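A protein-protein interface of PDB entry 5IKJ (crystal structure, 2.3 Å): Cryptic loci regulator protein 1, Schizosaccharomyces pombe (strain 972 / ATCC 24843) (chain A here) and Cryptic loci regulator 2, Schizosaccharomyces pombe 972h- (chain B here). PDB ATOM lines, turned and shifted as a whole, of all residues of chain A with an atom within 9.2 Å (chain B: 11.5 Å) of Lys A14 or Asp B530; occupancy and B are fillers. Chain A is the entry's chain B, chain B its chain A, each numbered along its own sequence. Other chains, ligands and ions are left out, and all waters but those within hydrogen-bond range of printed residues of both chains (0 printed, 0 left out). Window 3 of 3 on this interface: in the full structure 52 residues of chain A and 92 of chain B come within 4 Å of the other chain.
The side-chain carboxylate of Asp B530 is in salt-bridge range of the side-chain amino group of Lys A14. The side-chain carboxylate of Asp B530 is in salt-bridge range of the side-chain amino group of Lys A28 (2.6 Å).
Of chain B, only Asp B530 (3.0 Å) comes within 4 Å of Lys A14. Asp B530 touches just these residues of chain A: Lys A14 and Lys A28. No residue of chain B comes within 4 Å of Ser A13. No residue of chain B comes within 4 Å of Asp A15. Of chain B, only Tyr B533 (3.5 Å) and Leu B537 (3.7 Å) come within 4 Å of Ile A17. No residue of chain B comes within 4 Å of Ile A18. Of the printed residues of chain B, Tyr A34 touches Leu B519. Of the printed residues of chain A, Leu B537 touches Ile A17, Ala A20 and Leu A21. Trp B527 touches none of the printed residues of chain A. Ser B298 touches none of the printed residues of chain A. The nearest residue of chain A that does not touch Asp B530 is Ile A18 (6.1 Å).
Hydrophobic or aromatic side chains of chain B within 4 Å of the printed part of chain A: Leu B519, Tyr B533 and Leu B537. Of the 13 printed residues of chain A, 6 touch a printed residue of chain B. Printed residues of chain A that touch a printed residue of chain B: Lys A14, Ile A17, Ala A20, Leu A21, Lys A28 and Tyr A34. Hydrophobic or aromatic side chains of chain A within 4 Å of the printed part of chain B: Ile A17, Ala A20, Leu A21 and Tyr A34. Among the printed residues, Asp or Glu carboxylates within 4 Å of a Lys or Arg side-chain nitrogen of the other chain: Lys A14 with Asp B530 and Lys A28 with Asp B530.
Among the printed residues, pairs that only touch across the chains: Ile A17 with Tyr B533, Ile A17 with Leu B537, Ala A20 with Leu B537, Leu A21 with Tyr B533, Leu A21 with Leu B537, Lys A28 with Tyr B533 and Tyr A34 with Leu B519.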
ATOM      1  N   GLN A  12       8.709 -16.734  19.461  1.00  0.00           N
ATOM      2  CA  GLN A  12       7.378 -16.648  20.051  1.00  0.00           C
ATOM      3  C   GLN A  12       6.442 -15.823  19.176  1.00  0.00           C
ATOM      4  O   GLN A  12       5.256 -16.148  19.043  1.00  0.00           O
ATOM      5  CB  GLN A  12       7.475 -16.040  21.450  1.00  0.00           C
ATOM      6  CG  GLN A  12       6.342 -16.422  22.386  1.00  0.00           C
ATOM      7  CD  GLN A  12       6.574 -17.750  23.078  1.00  0.00           C
ATOM      8  OE1 GLN A  12       7.138 -18.679  22.497  1.00  0.00           O
ATOM      9  NE2 GLN A  12       6.147 -17.843  24.332  1.00  0.00           N
ATOM     10  N   SER A  13       6.958 -14.751  18.566  1.00  0.00           N
ATOM     11  CA  SER A  13       6.120 -13.870  17.761  1.00  0.00           C
ATOM     12  C   SER A  13       5.694 -14.515  16.449  1.00  0.00           C
ATOM     13  O   SER A  13       4.693 -14.091  15.863  1.00  0.00           O
ATOM     14  CB  SER A  13       6.858 -12.561  17.474  1.00  0.00           C
ATOM     15  OG  SER A  13       7.642 -12.663  16.298  1.00  0.00           O
ATOM     16  N   LYS A  14       6.431 -15.520  15.969  1.00  0.00           N
ATOM     17  CA  LYS A  14       6.014 -16.224  14.761  1.00  0.00           C
ATOM     18  C   LYS A  14       4.758 -17.049  15.005  1.00  0.00           C
ATOM     19  O   LYS A  14       3.918 -17.178  14.107  1.00  0.00           O
ATOM     20  CB  LYS A  14       7.139 -17.127  14.254  1.00  0.00           C
ATOM     21  CG  LYS A  14       8.448 -16.411  13.959  1.00  0.00           C
ATOM     22  CD  LYS A  14       9.056 -16.896  12.649  1.00  0.00           C
ATOM     23  CE  LYS A  14      10.541 -16.583  12.564  1.00  0.00           C
ATOM     24  NZ  LYS A  14      11.123 -17.039  11.272  1.00  0.00           N
ATOM     25  N   ASP A  15       4.611 -17.610  16.208  1.00  0.00           N
ATOM     26  CA  ASP A  15       3.443 -18.431  16.508  1.00  0.00           C
ATOM     27  C   ASP A  15       2.157 -17.615  16.480  1.00  0.00           C
ATOM     28  O   ASP A  15       1.094 -18.149  16.144  1.00  0.00           O
ATOM     29  CB  ASP A  15       3.614 -19.103  17.871  1.00  0.00           C
ATOM     30  CG  ASP A  15       4.755 -20.100  17.888  1.00  0.00           C
ATOM     31  OD1 ASP A  15       5.641 -20.008  17.012  1.00  0.00           O
ATOM     32  OD2 ASP A  15       4.768 -20.975  18.779  1.00  0.00           O
ATOM     33  N   LYS A  16       2.226 -16.328  16.829  1.00  0.00           N
ATOM     34  CA  LYS A  16       1.025 -15.501  16.844  1.00  0.00           C
ATOM     35  C   LYS A  16       0.612 -15.091  15.435  1.00  0.00           C
ATOM     36  O   LYS A  16      -0.584 -15.016  15.135  1.00  0.00           O
ATOM     37  CB  LYS A  16       1.248 -14.269  17.722  1.00  0.00           C
ATOM     38  CG  LYS A  16       1.507 -14.603  19.183  1.00  0.00           C
ATOM     39  CD  LYS A  16       1.552 -13.353  20.047  1.00  0.00           C
ATOM     40  CE  LYS A  16       1.815 -13.701  21.503  1.00  0.00           C
ATOM     41  NZ  LYS A  16       1.797 -12.500  22.382  1.00  0.00           N
ATOM     42  N   ILE A  17       1.583 -14.818  14.561  1.00  0.00           N
ATOM     43  CA  ILE A  17       1.267 -14.516  13.167  1.00  0.00           C
ATOM     44  C   ILE A  17       0.579 -15.710  12.517  1.00  0.00           C
ATOM     45  O   ILE A  17      -0.511 -15.589  11.945  1.00  0.00           O
ATOM     46  CB  ILE A  17       2.543 -14.116  12.402  1.00  0.00           C
ATOM     47  CG1 ILE A  17       3.169 -12.864  13.025  1.00  0.00           C
ATOM     48  CG2 ILE A  17       2.228 -13.878  10.927  1.00  0.00           C
ATOM     49  CD1 ILE A  17       4.509 -12.473  12.431  1.00  0.00           C
ATOM     50  N   ILE A  18       1.215 -16.882  12.591  1.00  0.00           N
ATOM     51  CA  ILE A  18       0.643 -18.096  12.010  1.00  0.00           C
ATOM     52  C   ILE A  18      -0.769 -18.321  12.534  1.00  0.00           C
ATOM     53  O   ILE A  18      -1.699 -18.603  11.768  1.00  0.00           O
ATOM     54  CB  ILE A  18       1.557 -19.300  12.302  1.00  0.00           C
ATOM     55  CG1 ILE A  18       2.817 -19.217  11.435  1.00  0.00           C
ATOM     56  CG2 ILE A  18       0.826 -20.622  12.064  1.00  0.00           C
ATOM     57  CD1 ILE A  18       3.918 -20.164  11.854  1.00  0.00           C
ATOM     58  N   ALA A  19      -0.952 -18.205  13.851  1.00  0.00           N
ATOM     59  CA  ALA A  19      -2.274 -18.411  14.433  1.00  0.00           C
ATOM     60  C   ALA A  19      -3.287 -17.424  13.866  1.00  0.00           C
ATOM     61  O   ALA A  19      -4.457 -17.770  13.665  1.00  0.00           O
ATOM     62  CB  ALA A  19      -2.202 -18.286  15.954  1.00  0.00           C
ATOM     63  N   ALA A  20      -2.856 -16.188  13.601  1.00  0.00           N
ATOM     64  CA  ALA A  20      -3.769 -15.191  13.054  1.00  0.00           C
ATOM     65  C   ALA A  20      -4.083 -15.476  11.590  1.00  0.00           C
ATOM     66  O   ALA A  20      -5.224 -15.293  11.147  1.00  0.00           O
ATOM     67  CB  ALA A  20      -3.174 -13.792  13.213  1.00  0.00           C
ATOM     68  N   LEU A  21      -3.087 -15.923  10.822  1.00  0.00           N
ATOM     69  CA  LEU A  21      -3.338 -16.297   9.435  1.00  0.00           C
ATOM     70  C   LEU A  21      -4.270 -17.499   9.344  1.00  0.00           C
ATOM     71  O   LEU A  21      -5.033 -17.620   8.379  1.00  0.00           O
ATOM     72  CB  LEU A  21      -2.018 -16.598   8.724  1.00  0.00           C
ATOM     73  CG  LEU A  21      -1.089 -15.404   8.493  1.00  0.00           C
ATOM     74  CD1 LEU A  21       0.265 -15.879   8.000  1.00  0.00           C
ATOM     75  CD2 LEU A  21      -1.694 -14.418   7.502  1.00  0.00           C
ATOM     76  N   ALA A  22      -4.224 -18.394  10.333  1.00  0.00           N
ATOM     77  CA  ALA A  22      -5.098 -19.561  10.314  1.00  0.00           C
ATOM     78  C   ALA A  22      -6.560 -19.167  10.468  1.00  0.00           C
ATOM     79  O   ALA A  22      -7.438 -19.815   9.885  1.00  0.00           O
ATOM     80  CB  ALA A  22      -4.691 -20.541  11.413  1.00  0.00           C
ATOM     81  N   LYS A  28       1.116 -22.087   5.832  1.00  0.00           N
ATOM     82  CA  LYS A  28       2.366 -22.277   5.106  1.00  0.00           C
ATOM     83  C   LYS A  28       2.359 -23.537   4.255  1.00  0.00           C
ATOM     84  O   LYS A  28       3.283 -23.731   3.458  1.00  0.00           O
ATOM     85  CB  LYS A  28       3.540 -22.332   6.086  1.00  0.00           C
ATOM     86  CG  LYS A  28       3.768 -21.048   6.863  1.00  0.00           C
ATOM     87  CD  LYS A  28       5.062 -21.119   7.656  1.00  0.00           C
ATOM     88  CE  LYS A  28       5.269 -19.877   8.505  1.00  0.00           C
ATOM     89  NZ  LYS A  28       6.475 -19.997   9.372  1.00  0.00           N
ATOM     90  N   TYR A  34       4.596 -30.368   0.108  1.00  0.00           N
ATOM     91  CA  TYR A  34       5.660 -31.162   0.704  1.00  0.00           C
ATOM     92  C   TYR A  34       5.462 -32.641   0.393  1.00  0.00           C
ATOM     93  O   TYR A  34       4.344 -33.103   0.154  1.00  0.00           O
ATOM     94  CB  TYR A  34       5.708 -30.958   2.220  1.00  0.00           C
ATOM     95  CG  TYR A  34       5.984 -29.534   2.646  1.00  0.00           C
ATOM     96  CD1 TYR A  34       7.267 -29.009   2.592  1.00  0.00           C
ATOM     97  CD2 TYR A  34       4.962 -28.719   3.111  1.00  0.00           C
ATOM     98  CE1 TYR A  34       7.524 -27.708   2.986  1.00  0.00           C
ATOM     99  CE2 TYR A  34       5.210 -27.417   3.507  1.00  0.00           C
ATOM    100  CZ  TYR A  34       6.492 -26.918   3.441  1.00  0.00           C
ATOM    101  OH  TYR A  34       6.744 -25.623   3.833  1.00  0.00           O
ATOM    102  N   VAL B 262       1.383 -18.596  -3.795  1.00  0.00           N
ATOM    103  CA  VAL B 262       1.796 -19.099  -2.489  1.00  0.00           C
ATOM    104  C   VAL B 262       0.638 -19.166  -1.497  1.00  0.00           C
ATOM    105  O   VAL B 262       0.601 -20.059  -0.653  1.00  0.00           O
ATOM    106  CB  VAL B 262       2.939 -18.224  -1.938  1.00  0.00           C
ATOM    107  CG1 VAL B 262       3.402 -18.752  -0.585  1.00  0.00           C
ATOM    108  CG2 VAL B 262       4.090 -18.166  -2.929  1.00  0.00           C
ATOM    109  N   ALA B 263      -0.299 -18.227  -1.557  1.00  0.00           N
ATOM    110  CA  ALA B 263      -1.371 -18.128  -0.574  1.00  0.00           C
ATOM    111  C   ALA B 263      -2.522 -17.386  -1.229  1.00  0.00           C
ATOM    112  O   ALA B 263      -2.383 -16.812  -2.311  1.00  0.00           O
ATOM    113  CB  ALA B 263      -0.902 -17.415   0.703  1.00  0.00           C
ATOM    114  N   LYS B 293       4.793 -15.218  -5.453  1.00  0.00           N
ATOM    115  CA  LYS B 293       6.245 -15.172  -5.347  1.00  0.00           C
ATOM    116  C   LYS B 293       6.803 -15.205  -6.759  1.00  0.00           C
ATOM    117  O   LYS B 293       6.596 -16.183  -7.483  1.00  0.00           O
ATOM    118  CB  LYS B 293       6.772 -16.357  -4.525  1.00  0.00           C
ATOM    119  CG  LYS B 293       8.270 -16.639  -4.659  1.00  0.00           C
ATOM    120  CD  LYS B 293       9.120 -15.518  -4.086  1.00  0.00           C
ATOM    121  CE  LYS B 293      10.587 -15.922  -4.014  1.00  0.00           C
ATOM    122  NZ  LYS B 293      11.114 -16.382  -5.328  1.00  0.00           N
ATOM    123  N   SER B 298      13.463 -12.655  -5.817  1.00  0.00           N
ATOM    124  CA  SER B 298      13.082 -12.728  -4.414  1.00  0.00           C
ATOM    125  C   SER B 298      11.867 -11.864  -4.103  1.00  0.00           C
ATOM    126  O   SER B 298      11.528 -11.688  -2.929  1.00  0.00           O
ATOM    127  CB  SER B 298      14.256 -12.309  -3.526  1.00  0.00           C
ATOM    128  OG  SER B 298      14.564 -10.936  -3.695  1.00  0.00           O
ATOM    129  N   TYR B 300       8.181 -10.527  -3.507  1.00  0.00           N
ATOM    130  CA  TYR B 300       6.817 -10.897  -3.176  1.00  0.00           C
ATOM    131  C   TYR B 300       5.861  -9.896  -3.814  1.00  0.00           C
ATOM    132  O   TYR B 300       6.192  -8.719  -3.984  1.00  0.00           O
ATOM    133  CB  TYR B 300       6.598 -10.918  -1.660  1.00  0.00           C
ATOM    134  CG  TYR B 300       7.588 -11.739  -0.859  1.00  0.00           C
ATOM    135  CD1 TYR B 300       8.430 -12.663  -1.470  1.00  0.00           C
ATOM    136  CD2 TYR B 300       7.671 -11.593   0.520  1.00  0.00           C
ATOM    137  CE1 TYR B 300       9.330 -13.410  -0.726  1.00  0.00           C
ATOM    138  CE2 TYR B 300       8.562 -12.335   1.270  1.00  0.00           C
ATOM    139  CZ  TYR B 300       9.389 -13.242   0.643  1.00  0.00           C
ATOM    140  OH  TYR B 300      10.278 -13.981   1.389  1.00  0.00           O
ATOM    141  N   PHE B 302       1.854  -9.085  -3.089  1.00  0.00           N
ATOM    142  CA  PHE B 302       0.657  -9.372  -2.317  1.00  0.00           C
ATOM    143  C   PHE B 302      -0.561  -8.684  -2.926  1.00  0.00           C
ATOM    144  O   PHE B 302      -0.449  -7.749  -3.722  1.00  0.00           O
ATOM    145  CB  PHE B 302       0.836  -8.919  -0.869  1.00  0.00           C
ATOM    146  CG  PHE B 302       2.047  -9.498  -0.196  1.00  0.00           C
ATOM    147  CD1 PHE B 302       3.295  -8.923  -0.372  1.00  0.00           C
ATOM    148  CD2 PHE B 302       1.936 -10.611   0.621  1.00  0.00           C
ATOM    149  CE1 PHE B 302       4.410  -9.450   0.247  1.00  0.00           C
ATOM    150  CE2 PHE B 302       3.049 -11.144   1.243  1.00  0.00           C
ATOM    151  CZ  PHE B 302       4.288 -10.562   1.056  1.00  0.00           C
ATOM    152  N   LEU B 519       7.252 -28.369  -3.868  1.00  0.00           N
ATOM    153  CA  LEU B 519       8.441 -27.689  -3.366  1.00  0.00           C
ATOM    154  C   LEU B 519       9.707 -28.257  -3.993  1.00  0.00           C
ATOM    155  O   LEU B 519      10.657 -27.516  -4.273  1.00  0.00           O
ATOM    156  CB  LEU B 519       8.500 -27.803  -1.842  1.00  0.00           C
ATOM    157  CG  LEU B 519       9.622 -27.036  -1.138  1.00  0.00           C
ATOM    158  CD1 LEU B 519       9.545 -25.547  -1.441  1.00  0.00           C
ATOM    159  CD2 LEU B 519       9.555 -27.270   0.363  1.00  0.00           C
ATOM    160  N   SER B 524      13.752 -24.913  -2.909  1.00  0.00           N
ATOM    161  CA  SER B 524      13.542 -24.104  -1.713  1.00  0.00           C
ATOM    162  C   SER B 524      14.128 -22.705  -1.865  1.00  0.00           C
ATOM    163  O   SER B 524      13.653 -21.763  -1.220  1.00  0.00           O
ATOM    164  CB  SER B 524      14.147 -24.802  -0.497  1.00  0.00           C
ATOM    165  OG  SER B 524      15.538 -24.996  -0.666  1.00  0.00           O
ATOM    166  N   GLU B 525      15.156 -22.545  -2.705  1.00  0.00           N
ATOM    167  CA  GLU B 525      15.715 -21.218  -2.939  1.00  0.00           C
ATOM    168  C   GLU B 525      14.750 -20.313  -3.694  1.00  0.00           C
ATOM    169  O   GLU B 525      14.900 -19.088  -3.643  1.00  0.00           O
ATOM    170  CB  GLU B 525      17.038 -21.309  -3.709  1.00  0.00           C
ATOM    171  CG  GLU B 525      16.945 -21.852  -5.134  1.00  0.00           C
ATOM    172  CD  GLU B 525      16.906 -23.366  -5.186  1.00  0.00           C
ATOM    173  OE1 GLU B 525      16.545 -23.990  -4.165  1.00  0.00           O
ATOM    174  OE2 GLU B 525      17.243 -23.935  -6.246  1.00  0.00           O
ATOM    175  N   ASN B 526      13.769 -20.888  -4.387  1.00  0.00           N
ATOM    176  CA  ASN B 526      12.790 -20.126  -5.148  1.00  0.00           C
ATOM    177  C   ASN B 526      11.457 -19.997  -4.425  1.00  0.00           C
ATOM    178  O   ASN B 526      10.555 -19.326  -4.935  1.00  0.00           O
ATOM    179  CB  ASN B 526      12.576 -20.778  -6.518  1.00  0.00           C
ATOM    180  CG  ASN B 526      13.833 -20.771  -7.368  1.00  0.00           C
ATOM    181  OD1 ASN B 526      14.450 -19.726  -7.571  1.00  0.00           O
ATOM    182  ND2 ASN B 526      14.226 -21.943  -7.858  1.00  0.00           N
ATOM    183  N   TRP B 527      11.313 -20.616  -3.257  1.00  0.00           N
ATOM    184  CA  TRP B 527      10.104 -20.507  -2.460  1.00  0.00           C
ATOM    185  C   TRP B 527      10.227 -19.274  -1.562  1.00  0.00           C
ATOM    186  O   TRP B 527      11.181 -18.499  -1.668  1.00  0.00           O
ATOM    187  CB  TRP B 527       9.883 -21.808  -1.687  1.00  0.00           C
ATOM    188  CG  TRP B 527       8.503 -21.987  -1.122  1.00  0.00           C
ATOM    189  CD1 TRP B 527       8.179 -22.246   0.178  1.00  0.00           C
ATOM    190  CD2 TRP B 527       7.261 -21.917  -1.836  1.00  0.00           C
ATOM    191  NE1 TRP B 527       6.817 -22.345   0.318  1.00  0.00           N
ATOM    192  CE2 TRP B 527       6.230 -22.146  -0.903  1.00  0.00           C
ATOM    193  CE3 TRP B 527       6.922 -21.681  -3.172  1.00  0.00           C
ATOM    194  CZ2 TRP B 527       4.884 -22.149  -1.263  1.00  0.00           C
ATOM    195  CZ3 TRP B 527       5.583 -21.683  -3.527  1.00  0.00           C
ATOM    196  CH2 TRP B 527       4.582 -21.915  -2.576  1.00  0.00           C
ATOM    197  N   VAL B 528       9.264 -19.070  -0.671  1.00  0.00           N
ATOM    198  CA  VAL B 528       9.225 -17.871   0.151  1.00  0.00           C
ATOM    199  C   VAL B 528       9.928 -18.132   1.477  1.00  0.00           C
ATOM    200  O   VAL B 528      10.146 -19.275   1.886  1.00  0.00           O
ATOM    201  CB  VAL B 528       7.776 -17.394   0.381  1.00  0.00           C
ATOM    202  CG1 VAL B 528       7.119 -17.042  -0.943  1.00  0.00           C
ATOM    203  CG2 VAL B 528       6.965 -18.454   1.123  1.00  0.00           C
ATOM    204  N   ASP B 529      10.287 -17.047   2.157  1.00  0.00           N
ATOM    205  CA  ASP B 529      10.822 -17.101   3.508  1.00  0.00           C
ATOM    206  C   ASP B 529       9.736 -16.711   4.506  1.00  0.00           C
ATOM    207  O   ASP B 529       8.668 -16.215   4.139  1.00  0.00           O
ATOM    208  CB  ASP B 529      12.040 -16.182   3.643  1.00  0.00           C
ATOM    209  CG  ASP B 529      13.146 -16.533   2.665  1.00  0.00           C
ATOM    210  OD1 ASP B 529      12.833 -17.045   1.569  1.00  0.00           O
ATOM    211  OD2 ASP B 529      14.327 -16.294   2.991  1.00  0.00           O
ATOM    212  N   ASP B 530      10.023 -16.938   5.789  1.00  0.00           N
ATOM    213  CA  ASP B 530       9.014 -16.726   6.823  1.00  0.00           C
ATOM    214  C   ASP B 530       8.511 -15.289   6.874  1.00  0.00           C
ATOM    215  O   ASP B 530       7.405 -15.052   7.372  1.00  0.00           O
ATOM    216  CB  ASP B 530       9.568 -17.127   8.193  1.00  0.00           C
ATOM    217  CG  ASP B 530       9.415 -18.610   8.476  1.00  0.00           C
ATOM    218  OD1 ASP B 530       8.498 -19.239   7.905  1.00  0.00           O
ATOM    219  OD2 ASP B 530      10.208 -19.148   9.277  1.00  0.00           O
ATOM    220  N   ASP B 531       9.289 -14.323   6.380  1.00  0.00           N
ATOM    221  CA  ASP B 531       8.828 -12.938   6.390  1.00  0.00           C
ATOM    222  C   ASP B 531       7.593 -12.758   5.516  1.00  0.00           C
ATOM    223  O   ASP B 531       6.740 -11.913   5.815  1.00  0.00           O
ATOM    224  CB  ASP B 531       9.946 -12.009   5.921  1.00  0.00           C
ATOM    225  CG  ASP B 531      10.433 -12.345   4.528  1.00  0.00           C
ATOM    226  OD1 ASP B 531      10.326 -13.525   4.135  1.00  0.00           O
ATOM    227  OD2 ASP B 531      10.920 -11.433   3.827  1.00  0.00           O
ATOM    228  N   PHE B 532       7.488 -13.535   4.435  1.00  0.00           N
ATOM    229  CA  PHE B 532       6.313 -13.507   3.569  1.00  0.00           C
ATOM    230  C   PHE B 532       5.020 -13.472   4.373  1.00  0.00           C
ATOM    231  O   PHE B 532       4.128 -12.659   4.107  1.00  0.00           O
ATOM    232  CB  PHE B 532       6.337 -14.733   2.655  1.00  0.00           C
ATOM    233  CG  PHE B 532       5.234 -14.760   1.633  1.00  0.00           C
ATOM    234  CD1 PHE B 532       4.005 -15.325   1.932  1.00  0.00           C
ATOM    235  CD2 PHE B 532       5.435 -14.236   0.367  1.00  0.00           C
ATOM    236  CE1 PHE B 532       2.995 -15.357   0.990  1.00  0.00           C
ATOM    237  CE2 PHE B 532       4.429 -14.265  -0.578  1.00  0.00           C
ATOM    238  CZ  PHE B 532       3.208 -14.827  -0.267  1.00  0.00           C
ATOM    239  N   TYR B 533       4.907 -14.353   5.365  1.00  0.00           N
ATOM    240  CA  TYR B 533       3.670 -14.484   6.121  1.00  0.00           C
ATOM    241  C   TYR B 533       3.500 -13.386   7.161  1.00  0.00           C
ATOM    242  O   TYR B 533       2.365 -13.098   7.556  1.00  0.00           O
ATOM    243  CB  TYR B 533       3.624 -15.869   6.769  1.00  0.00           C
ATOM    244  CG  TYR B 533       3.703 -16.972   5.743  1.00  0.00           C
ATOM    245  CD1 TYR B 533       2.560 -17.435   5.104  1.00  0.00           C
ATOM    246  CD2 TYR B 533       4.923 -17.529   5.388  1.00  0.00           C
ATOM    247  CE1 TYR B 533       2.629 -18.434   4.154  1.00  0.00           C
ATOM    248  CE2 TYR B 533       5.003 -18.528   4.438  1.00  0.00           C
ATOM    249  CZ  TYR B 533       3.852 -18.976   3.823  1.00  0.00           C
ATOM    250  OH  TYR B 533       3.926 -19.971   2.878  1.00  0.00           O
ATOM    251  N   GLU B 534       4.587 -12.698   7.489  1.00  0.00           N
ATOM    252  CA  GLU B 534       4.517 -11.546   8.365  1.00  0.00           C
ATOM    253  C   GLU B 534       3.897 -10.445   7.499  1.00  0.00           C
ATOM    254  O   GLU B 534       2.891  -9.857   7.867  1.00  0.00           O
ATOM    255  CB  GLU B 534       5.899 -11.144   8.868  1.00  0.00           C
ATOM    256  CG  GLU B 534       5.907  -9.849   9.660  1.00  0.00           C
ATOM    257  CD  GLU B 534       7.015  -9.789  10.691  1.00  0.00           C
ATOM    258  OE1 GLU B 534       8.050 -10.456  10.505  1.00  0.00           O
ATOM    259  OE2 GLU B 534       6.846  -9.067  11.691  1.00  0.00           O
ATOM    260  N   TYR B 535       4.496 -10.188   6.336  1.00  0.00           N
ATOM    261  CA  TYR B 535       3.959  -9.210   5.396  1.00  0.00           C
ATOM    262  C   TYR B 535       2.503  -9.512   5.062  1.00  0.00           C
ATOM    263  O   TYR B 535       1.643  -8.624   5.118  1.00  0.00           O
ATOM    264  CB  TYR B 535       4.799  -9.192   4.117  1.00  0.00           C
ATOM    265  CG  TYR B 535       6.212  -8.688   4.299  1.00  0.00           C
ATOM    266  CD1 TYR B 535       6.459  -7.371   4.664  1.00  0.00           C
ATOM    267  CD2 TYR B 535       7.299  -9.524   4.088  1.00  0.00           C
ATOM    268  CE1 TYR B 535       7.751  -6.905   4.825  1.00  0.00           C
ATOM    269  CE2 TYR B 535       8.593  -9.068   4.244  1.00  0.00           C
ATOM    270  CZ  TYR B 535       8.814  -7.757   4.613  1.00  0.00           C
ATOM    271  OH  TYR B 535      10.103  -7.303   4.770  1.00  0.00           O
ATOM    272  N   LEU B 536       2.212 -10.766   4.708  1.00  0.00           N
ATOM    273  CA  LEU B 536       0.859 -11.141   4.305  1.00  0.00           C
ATOM    274  C   LEU B 536      -0.156 -10.743   5.368  1.00  0.00           C
ATOM    275  O   LEU B 536      -1.173 -10.109   5.066  1.00  0.00           O
ATOM    276  CB  LEU B 536       0.794 -12.646   4.031  1.00  0.00           C
ATOM    277  CG  LEU B 536      -0.328 -13.149   3.116  1.00  0.00           C
ATOM    278  CD1 LEU B 536      -0.148 -14.633   2.831  1.00  0.00           C
ATOM    279  CD2 LEU B 536      -1.709 -12.903   3.702  1.00  0.00           C
ATOM    280  N   LEU B 537       0.109 -11.115   6.608  1.00  0.00           N
ATOM    281  CA  LEU B 537      -0.807 -10.806   7.688  1.00  0.00           C
ATOM    282  C   LEU B 537      -1.134  -9.326   7.744  1.00  0.00           C
ATOM    283  O   LEU B 537      -2.271  -8.945   7.987  1.00  0.00           O
ATOM    284  CB  LEU B 537      -0.239 -11.263   9.023  1.00  0.00           C
ATOM    285  CG  LEU B 537      -1.186 -11.017  10.185  1.00  0.00           C
ATOM    286  CD1 LEU B 537      -2.572 -11.507   9.828  1.00  0.00           C
ATOM    287  CD2 LEU B 537      -0.688 -11.687  11.448  1.00  0.00           C
ATOM    288  N   SER B 538      -0.131  -8.494   7.517  1.00  0.00           N
ATOM    289  CA  SER B 538      -0.327  -7.058   7.557  1.00  0.00           C
ATOM    290  C   SER B 538      -1.118  -6.587   6.363  1.00  0.00           C
ATOM    291  O   SER B 538      -1.876  -5.633   6.451  1.00  0.00           O
ATOM    292  CB  SER B 538       1.017  -6.340   7.580  1.00  0.00           C
ATOM    293  OG  SER B 538       1.688  -6.571   8.795  1.00  0.00           O
